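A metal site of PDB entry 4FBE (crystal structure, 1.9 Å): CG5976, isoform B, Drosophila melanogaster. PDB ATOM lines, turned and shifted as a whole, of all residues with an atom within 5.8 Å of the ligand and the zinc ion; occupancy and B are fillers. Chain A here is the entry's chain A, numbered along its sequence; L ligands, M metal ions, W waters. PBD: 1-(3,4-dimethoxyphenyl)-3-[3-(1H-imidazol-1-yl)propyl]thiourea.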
ATOM      1  N   HIS A 113      -4.086 -10.082  19.082  1.00  0.00           N
ATOM      2  CA  HIS A 113      -3.642  -9.135  20.115  1.00  0.00           C
ATOM      3  C   HIS A 113      -2.938  -7.941  19.462  1.00  0.00           C
ATOM      4  O   HIS A 113      -2.198  -8.100  18.495  1.00  0.00           O
ATOM      5  CB  HIS A 113      -2.773  -9.796  21.184  1.00  0.00           C
ATOM      6  CG  HIS A 113      -1.360 -10.017  20.747  1.00  0.00           C
ATOM      7  ND1 HIS A 113      -0.387  -9.040  20.882  1.00  0.00           N
ATOM      8  CD2 HIS A 113      -0.761 -11.074  20.148  1.00  0.00           C
ATOM      9  CE1 HIS A 113       0.749  -9.500  20.378  1.00  0.00           C
ATOM     10  NE2 HIS A 113       0.553 -10.730  19.951  1.00  0.00           N
ATOM     11  N   LYS A 117       5.382  -6.791  22.382  1.00  0.00           N
ATOM     12  CA  LYS A 117       6.184  -7.267  23.510  1.00  0.00           C
ATOM     13  C   LYS A 117       7.177  -6.199  23.964  1.00  0.00           C
ATOM     14  O   LYS A 117       7.846  -5.577  23.158  1.00  0.00           O
ATOM     15  CB  LYS A 117       6.955  -8.537  23.141  1.00  0.00           C
ATOM     16  CG  LYS A 117       7.720  -9.217  24.321  1.00  0.00           C
ATOM     17  CD  LYS A 117       8.043 -10.692  24.003  1.00  0.00           C
ATOM     18  CE  LYS A 117       8.920 -11.385  25.076  1.00  0.00           C
ATOM     19  NZ  LYS A 117       8.362 -11.279  26.429  1.00  0.00           N
ATOM     20  N   PHE A 124      10.895  -3.504  19.184  1.00  0.00           N
ATOM     21  CA  PHE A 124      10.266  -4.704  18.673  1.00  0.00           C
ATOM     22  C   PHE A 124       8.941  -4.320  18.023  1.00  0.00           C
ATOM     23  O   PHE A 124       8.102  -3.709  18.659  1.00  0.00           O
ATOM     24  CB  PHE A 124      10.019  -5.691  19.826  1.00  0.00           C
ATOM     25  CG  PHE A 124       9.397  -6.977  19.391  1.00  0.00           C
ATOM     26  CD1 PHE A 124      10.092  -7.835  18.569  1.00  0.00           C
ATOM     27  CD2 PHE A 124       8.123  -7.321  19.788  1.00  0.00           C
ATOM     28  CE1 PHE A 124       9.522  -9.033  18.143  1.00  0.00           C
ATOM     29  CE2 PHE A 124       7.549  -8.532  19.360  1.00  0.00           C
ATOM     30  CZ  PHE A 124       8.244  -9.370  18.551  1.00  0.00           C
ATOM     31  N   ASP A 129       3.402 -10.791  14.970  1.00  0.00           N
ATOM     32  CA  ASP A 129       3.042 -10.981  16.362  1.00  0.00           C
ATOM     33  C   ASP A 129       2.643  -9.674  17.080  1.00  0.00           C
ATOM     34  O   ASP A 129       3.389  -9.180  17.928  1.00  0.00           O
ATOM     35  CB  ASP A 129       4.275 -11.578  17.059  1.00  0.00           C
ATOM     36  CG  ASP A 129       4.017 -12.026  18.487  1.00  0.00           C
ATOM     37  OD1 ASP A 129       2.839 -12.012  18.942  1.00  0.00           O
ATOM     38  OD2 ASP A 129       5.003 -12.377  19.175  1.00  0.00           O
ATOM     39  N   GLU A 166      -1.248  -9.268  25.588  1.00  0.00           N
ATOM     40  CA  GLU A 166      -1.026 -10.690  25.383  1.00  0.00           C
ATOM     41  C   GLU A 166       0.361 -11.067  25.863  1.00  0.00           C
ATOM     42  O   GLU A 166       0.536 -12.144  26.438  1.00  0.00           O
ATOM     43  CB  GLU A 166      -1.266 -11.088  23.947  1.00  0.00           C
ATOM     44  CG  GLU A 166      -1.169 -12.598  23.641  1.00  0.00           C
ATOM     45  CD  GLU A 166       0.244 -13.081  23.293  1.00  0.00           C
ATOM     46  OE1 GLU A 166       1.211 -12.285  23.368  1.00  0.00           O
ATOM     47  OE2 GLU A 166       0.359 -14.261  22.908  1.00  0.00           O
ATOM     48  N   GLU A 167       1.324 -10.161  25.671  1.00  0.00           N
ATOM     49  CA  GLU A 167       2.729 -10.461  25.886  1.00  0.00           C
ATOM     50  C   GLU A 167       3.140 -10.243  27.312  1.00  0.00           C
ATOM     51  O   GLU A 167       2.568  -9.416  28.032  1.00  0.00           O
ATOM     52  CB  GLU A 167       3.620  -9.594  24.981  1.00  0.00           C
ATOM     53  CG  GLU A 167       3.343  -9.761  23.537  1.00  0.00           C
ATOM     54  CD  GLU A 167       4.042 -10.979  22.919  1.00  0.00           C
ATOM     55  OE1 GLU A 167       4.518 -11.892  23.637  1.00  0.00           O
ATOM     56  OE2 GLU A 167       4.097 -11.011  21.712  1.00  0.00           O
ATOM     57  N   TRP A 172       7.231 -15.103  30.526  1.00  0.00           N
ATOM     58  CA  TRP A 172       5.909 -15.639  30.212  1.00  0.00           C
ATOM     59  C   TRP A 172       5.482 -16.681  31.234  1.00  0.00           C
ATOM     60  O   TRP A 172       6.080 -17.751  31.328  1.00  0.00           O
ATOM     61  CB  TRP A 172       5.896 -16.268  28.821  1.00  0.00           C
ATOM     62  CG  TRP A 172       4.554 -16.812  28.437  1.00  0.00           C
ATOM     63  CD1 TRP A 172       4.014 -18.015  28.803  1.00  0.00           C
ATOM     64  CD2 TRP A 172       3.590 -16.180  27.589  1.00  0.00           C
ATOM     65  NE1 TRP A 172       2.759 -18.154  28.261  1.00  0.00           N
ATOM     66  CE2 TRP A 172       2.480 -17.048  27.500  1.00  0.00           C
ATOM     67  CE3 TRP A 172       3.542 -14.952  26.912  1.00  0.00           C
ATOM     68  CZ2 TRP A 172       1.341 -16.739  26.743  1.00  0.00           C
ATOM     69  CZ3 TRP A 172       2.410 -14.652  26.163  1.00  0.00           C
ATOM     70  CH2 TRP A 172       1.335 -15.538  26.087  1.00  0.00           C
ATOM     71  N   ASP A 204      -2.673 -15.614  15.222  1.00  0.00           N
ATOM     72  CA  ASP A 204      -1.398 -15.221  15.804  1.00  0.00           C
ATOM     73  C   ASP A 204      -0.220 -15.739  14.959  1.00  0.00           C
ATOM     74  O   ASP A 204      -0.296 -16.793  14.311  1.00  0.00           O
ATOM     75  CB  ASP A 204      -1.313 -15.767  17.224  1.00  0.00           C
ATOM     76  CG  ASP A 204      -0.340 -14.993  18.091  1.00  0.00           C
ATOM     77  OD1 ASP A 204       0.273 -14.046  17.582  1.00  0.00           O
ATOM     78  OD2 ASP A 204      -0.215 -15.328  19.286  1.00  0.00           O
ATOM     79  N   LEU A 205       0.856 -14.970  14.974  1.00  0.00           N
ATOM     80  CA  LEU A 205       2.078 -15.289  14.259  1.00  0.00           C
ATOM     81  C   LEU A 205       1.855 -15.528  12.755  1.00  0.00           C
ATOM     82  O   LEU A 205       2.329 -16.515  12.194  1.00  0.00           O
ATOM     83  CB  LEU A 205       2.768 -16.490  14.922  1.00  0.00           C
ATOM     84  CG  LEU A 205       2.970 -16.312  16.428  1.00  0.00           C
ATOM     85  CD1 LEU A 205       3.815 -17.406  16.998  1.00  0.00           C
ATOM     86  CD2 LEU A 205       3.573 -14.944  16.777  1.00  0.00           C
ATOM     87  N   PHE A 266      -0.602 -27.801  24.008  1.00  0.00           N
ATOM     88  CA  PHE A 266      -0.773 -26.829  25.101  1.00  0.00           C
ATOM     89  C   PHE A 266      -0.096 -25.483  24.844  1.00  0.00           C
ATOM     90  O   PHE A 266       0.510 -24.896  25.745  1.00  0.00           O
ATOM     91  CB  PHE A 266      -0.273 -27.400  26.445  1.00  0.00           C
ATOM     92  CG  PHE A 266      -0.990 -28.656  26.875  1.00  0.00           C
ATOM     93  CD1 PHE A 266      -2.355 -28.633  27.160  1.00  0.00           C
ATOM     94  CD2 PHE A 266      -0.299 -29.858  27.007  1.00  0.00           C
ATOM     95  CE1 PHE A 266      -3.022 -29.781  27.572  1.00  0.00           C
ATOM     96  CE2 PHE A 266      -0.960 -31.015  27.416  1.00  0.00           C
ATOM     97  CZ  PHE A 266      -2.322 -30.976  27.694  1.00  0.00           C
ATOM     98  N   ILE A 267      -0.237 -24.974  23.629  1.00  0.00           N
ATOM     99  CA  ILE A 267       0.285 -23.666  23.283  1.00  0.00           C
ATOM    100  C   ILE A 267      -0.553 -22.637  24.029  1.00  0.00           C
ATOM    101  O   ILE A 267      -1.801 -22.679  23.993  1.00  0.00           O
ATOM    102  CB  ILE A 267       0.270 -23.445  21.749  1.00  0.00           C
ATOM    103  CG1 ILE A 267       1.280 -24.388  21.087  1.00  0.00           C
ATOM    104  CG2 ILE A 267       0.613 -22.020  21.403  1.00  0.00           C
ATOM    105  CD1 ILE A 267       1.234 -24.401  19.548  1.00  0.00           C
ATOM    106  N   GLU A 268       0.105 -21.760  24.758  1.00  0.00           N
ATOM    107  CA  GLU A 268      -0.580 -20.748  25.564  1.00  0.00           C
ATOM    108  C   GLU A 268      -0.699 -19.447  24.755  1.00  0.00           C
ATOM    109  O   GLU A 268       0.226 -19.043  24.064  1.00  0.00           O
ATOM    110  CB  GLU A 268       0.170 -20.530  26.866  1.00  0.00           C
ATOM    111  CG  GLU A 268       0.356 -21.844  27.655  1.00  0.00           C
ATOM    112  CD  GLU A 268       0.881 -21.659  29.061  1.00  0.00           C
ATOM    113  OE1 GLU A 268       1.244 -20.526  29.471  1.00  0.00           O
ATOM    114  OE2 GLU A 268       0.899 -22.687  29.775  1.00  0.00           O
ATOM    115  N   ASP A 269      -1.857 -18.815  24.841  1.00  0.00           N
ATOM    116  CA  ASP A 269      -2.165 -17.607  24.080  1.00  0.00           C
ATOM    117  C   ASP A 269      -3.480 -17.028  24.626  1.00  0.00           C
ATOM    118  O   ASP A 269      -3.985 -17.492  25.643  1.00  0.00           O
ATOM    119  CB  ASP A 269      -2.270 -17.957  22.594  1.00  0.00           C
ATOM    120  CG  ASP A 269      -1.978 -16.809  21.678  1.00  0.00           C
ATOM    121  OD1 ASP A 269      -1.869 -15.647  22.114  1.00  0.00           O
ATOM    122  OD2 ASP A 269      -1.899 -17.068  20.481  1.00  0.00           O
ATOM    123  N   ILE A 285      -2.551 -20.397  14.366  1.00  0.00           N
ATOM    124  CA  ILE A 285      -1.193 -20.088  14.719  1.00  0.00           C
ATOM    125  C   ILE A 285      -0.323 -21.200  14.149  1.00  0.00           C
ATOM    126  O   ILE A 285      -0.621 -22.362  14.369  1.00  0.00           O
ATOM    127  CB  ILE A 285      -1.004 -19.983  16.245  1.00  0.00           C
ATOM    128  CG1 ILE A 285       0.408 -19.498  16.550  1.00  0.00           C
ATOM    129  CG2 ILE A 285      -1.262 -21.363  16.965  1.00  0.00           C
ATOM    130  CD1 ILE A 285       0.581 -19.144  17.997  1.00  0.00           C
ATOM    131  N   PRO A 286       0.764 -20.831  13.422  1.00  0.00           N
ATOM    132  CA  PRO A 286       1.561 -21.886  12.779  1.00  0.00           C
ATOM    133  C   PRO A 286       2.458 -22.651  13.755  1.00  0.00           C
ATOM    134  O   PRO A 286       2.825 -22.129  14.808  1.00  0.00           O
ATOM    135  CB  PRO A 286       2.405 -21.116  11.761  1.00  0.00           C
ATOM    136  CG  PRO A 286       2.273 -19.645  12.085  1.00  0.00           C
ATOM    137  CD  PRO A 286       1.373 -19.506  13.272  1.00  0.00           C
ATOM    138  N   VAL A 287       2.760 -23.904  13.406  1.00  0.00           N
ATOM    139  CA  VAL A 287       3.699 -24.746  14.119  1.00  0.00           C
ATOM    140  C   VAL A 287       4.584 -25.406  13.061  1.00  0.00           C
ATOM    141  O   VAL A 287       4.071 -26.160  12.242  1.00  0.00           O
ATOM    142  CB  VAL A 287       2.988 -25.850  14.921  1.00  0.00           C
ATOM    143  CG1 VAL A 287       3.981 -26.741  15.629  1.00  0.00           C
ATOM    144  CG2 VAL A 287       1.983 -25.244  15.944  1.00  0.00           C
ATOM    145  N   PRO A 288       5.909 -25.113  13.048  1.00  0.00           N
ATOM    146  CA  PRO A 288       6.594 -24.216  13.961  1.00  0.00           C
ATOM    147  C   PRO A 288       6.212 -22.738  13.827  1.00  0.00           C
ATOM    148  O   PRO A 288       5.730 -22.299  12.775  1.00  0.00           O
ATOM    149  CB  PRO A 288       8.085 -24.426  13.628  1.00  0.00           C
ATOM    150  CG  PRO A 288       8.071 -24.866  12.198  1.00  0.00           C
ATOM    151  CD  PRO A 288       6.837 -25.688  12.050  1.00  0.00           C
ATOM    152  N   PHE A 289       6.429 -21.991  14.905  1.00  0.00           N
ATOM    153  CA  PHE A 289       6.323 -20.535  14.917  1.00  0.00           C
ATOM    154  C   PHE A 289       7.381 -20.032  13.961  1.00  0.00           C
ATOM    155  O   PHE A 289       8.389 -20.692  13.756  1.00  0.00           O
ATOM    156  CB  PHE A 289       6.701 -19.963  16.284  1.00  0.00           C
ATOM    157  CG  PHE A 289       5.688 -20.194  17.372  1.00  0.00           C
ATOM    158  CD1 PHE A 289       4.605 -21.051  17.209  1.00  0.00           C
ATOM    159  CD2 PHE A 289       5.855 -19.571  18.589  1.00  0.00           C
ATOM    160  CE1 PHE A 289       3.710 -21.266  18.234  1.00  0.00           C
ATOM    161  CE2 PHE A 289       4.951 -19.771  19.628  1.00  0.00           C
ATOM    162  CZ  PHE A 289       3.878 -20.608  19.457  1.00  0.00           C
ATOM    163  N   TRP A 293      10.432 -15.346  15.522  1.00  0.00           N
ATOM    164  CA  TRP A 293       9.631 -15.155  16.746  1.00  0.00           C
ATOM    165  C   TRP A 293      10.403 -14.505  17.903  1.00  0.00           C
ATOM    166  O   TRP A 293      11.484 -14.960  18.275  1.00  0.00           O
ATOM    167  CB  TRP A 293       9.042 -16.503  17.186  1.00  0.00           C
ATOM    168  CG  TRP A 293       8.079 -16.417  18.331  1.00  0.00           C
ATOM    169  CD1 TRP A 293       6.793 -15.942  18.294  1.00  0.00           C
ATOM    170  CD2 TRP A 293       8.324 -16.824  19.683  1.00  0.00           C
ATOM    171  NE1 TRP A 293       6.231 -16.021  19.556  1.00  0.00           N
ATOM    172  CE2 TRP A 293       7.151 -16.562  20.414  1.00  0.00           C
ATOM    173  CE3 TRP A 293       9.428 -17.383  20.341  1.00  0.00           C
ATOM    174  CZ2 TRP A 293       7.053 -16.836  21.779  1.00  0.00           C
ATOM    175  CZ3 TRP A 293       9.319 -17.658  21.687  1.00  0.00           C
ATOM    176  CH2 TRP A 293       8.151 -17.387  22.389  1.00  0.00           C
ATOM    177  N   HIS A 294       9.840 -13.430  18.470  1.00  0.00           N
ATOM    178  CA  HIS A 294      10.443 -12.681  19.583  1.00  0.00           C
ATOM    179  C   HIS A 294      11.900 -12.245  19.373  1.00  0.00           C
ATOM    180  O   HIS A 294      12.666 -12.158  20.314  1.00  0.00           O
ATOM    181  CB  HIS A 294      10.270 -13.458  20.904  1.00  0.00           C
ATOM    182  CG  HIS A 294       8.848 -13.505  21.379  1.00  0.00           C
ATOM    183  ND1 HIS A 294       8.476 -14.042  22.592  1.00  0.00           N
ATOM    184  CD2 HIS A 294       7.725 -13.025  20.802  1.00  0.00           C
ATOM    185  CE1 HIS A 294       7.162 -13.914  22.725  1.00  0.00           C
ATOM    186  NE2 HIS A 294       6.692 -13.308  21.659  1.00  0.00           N
HETATM  187  CAA PBD L   1       9.819 -21.588  19.721  1.00  0.00           C
HETATM  188  CAB PBD L   1       5.308 -24.575  19.310  1.00  0.00           C
HETATM  189  SAC PBD L   1       3.453 -22.016  25.771  1.00  0.00           S
HETATM  190  CAD PBD L   1       2.714 -15.189  20.428  1.00  0.00           C
HETATM  191  CAE PBD L   1       7.028 -21.548  22.822  1.00  0.00           C
HETATM  192  CAF PBD L   1       7.845 -21.326  21.716  1.00  0.00           C
HETATM  193  CAG PBD L   1       2.385 -16.265  21.146  1.00  0.00           C
HETATM  194  CAH PBD L   1       3.584 -14.953  22.402  1.00  0.00           C
HETATM  195  CAI PBD L   1       5.791 -23.215  21.603  1.00  0.00           C
HETATM  196  CAJ PBD L   1       3.131 -18.464  22.994  1.00  0.00           C
HETATM  197  CAK PBD L   1       3.331 -19.469  24.129  1.00  0.00           C
HETATM  198  CAL PBD L   1       2.803 -17.050  23.506  1.00  0.00           C
HETATM  199  NAM PBD L   1       3.448 -14.374  21.209  1.00  0.00           N
HETATM  200  NAN PBD L   1       4.240 -20.546  23.662  1.00  0.00           N
HETATM  201  NAO PBD L   1       5.229 -22.658  23.850  1.00  0.00           N
HETATM  202  OAP PBD L   1       8.440 -21.823  19.455  1.00  0.00           O
HETATM  203  OAQ PBD L   1       6.456 -23.674  19.309  1.00  0.00           O
HETATM  204  CAR PBD L   1       4.396 -21.703  24.317  1.00  0.00           C
HETATM  205  CAS PBD L   1       5.996 -22.486  22.772  1.00  0.00           C
HETATM  206  CAT PBD L   1       7.649 -22.050  20.546  1.00  0.00           C
HETATM  207  CAU PBD L   1       6.621 -22.994  20.485  1.00  0.00           C
HETATM  208  NAV PBD L   1       2.910 -16.085  22.378  1.00  0.00           N
HETATM  209 ZN    ZN M   1       4.765 -12.714  20.986  1.00  0.00          ZN
HETATM  210  O   HOH W   1       8.019 -23.412  17.228  1.00  0.00           O
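N of Glu 268 sits close to SAC of the ligand.
The indole nitrogen of Trp 293 sits close to a ring nitrogen (NE2) of His 294, at 3.5 Å. The side-chain carboxylate of Asp 204 lies close to the side-chain carboxylate of Asp 269 (2.7 Å). The side-chain carboxylate (OD1) of Asp 269 sits close to the side-chain carboxylate (OE2) of Glu 166. OD1 of Asp 129 is in hydrogen-bond range of NE2 of His 113 (2.8 Å). OE1 of Glu 268 sits at hydrogen-bond distance from NE1 of Trp 172, at 3.1 Å.
NAV of the ligand sits close to OE2 of Glu 166. Trp 172 touches the ligand. Asp 204 touches the ligand. Leu 205 touches the ligand. Phe 289 touches the ligand. Trp 293 touches the ligand. Hydrophobic or aromatic side chains that line the ligand: Trp 172, Leu 205, Phe 289, Trp 293 and His 294. Ten residues have an atom within 4 Å of the ligand: Asp 129, Glu 166, Glu 167, Trp 172, Asp 204, Leu 205, Glu 268, Phe 289, Trp 293 and His 294. The nearest printed residue that does not touch the ligand is Ile 267 (4.1 Å).
NE1 of Trp 293 touches the zinc ion, at 3.9 Å. The nearest printed residue that does not touch the zinc ion is Glu 166 (4.3 Å).
The zinc ion is bound by the side-chain carboxylate (OD2) of Asp 129 (1.9 Å), the side-chain carboxylate (OE2) of Glu 167 (2.0 Å), a ring nitrogen (NE2) of His 294 (2.1 Å) and a nitrogen (NAM) of the ligand (2.1 Å). Slightly farther from the zinc ion lies the side-chain carboxylate (OE1) of Glu 167 (2.8 Å).
Water W1 lies within hydrogen-bond range of OAQ of the ligand (2.6 Å) and N of Phe 289 (3.2 Å).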
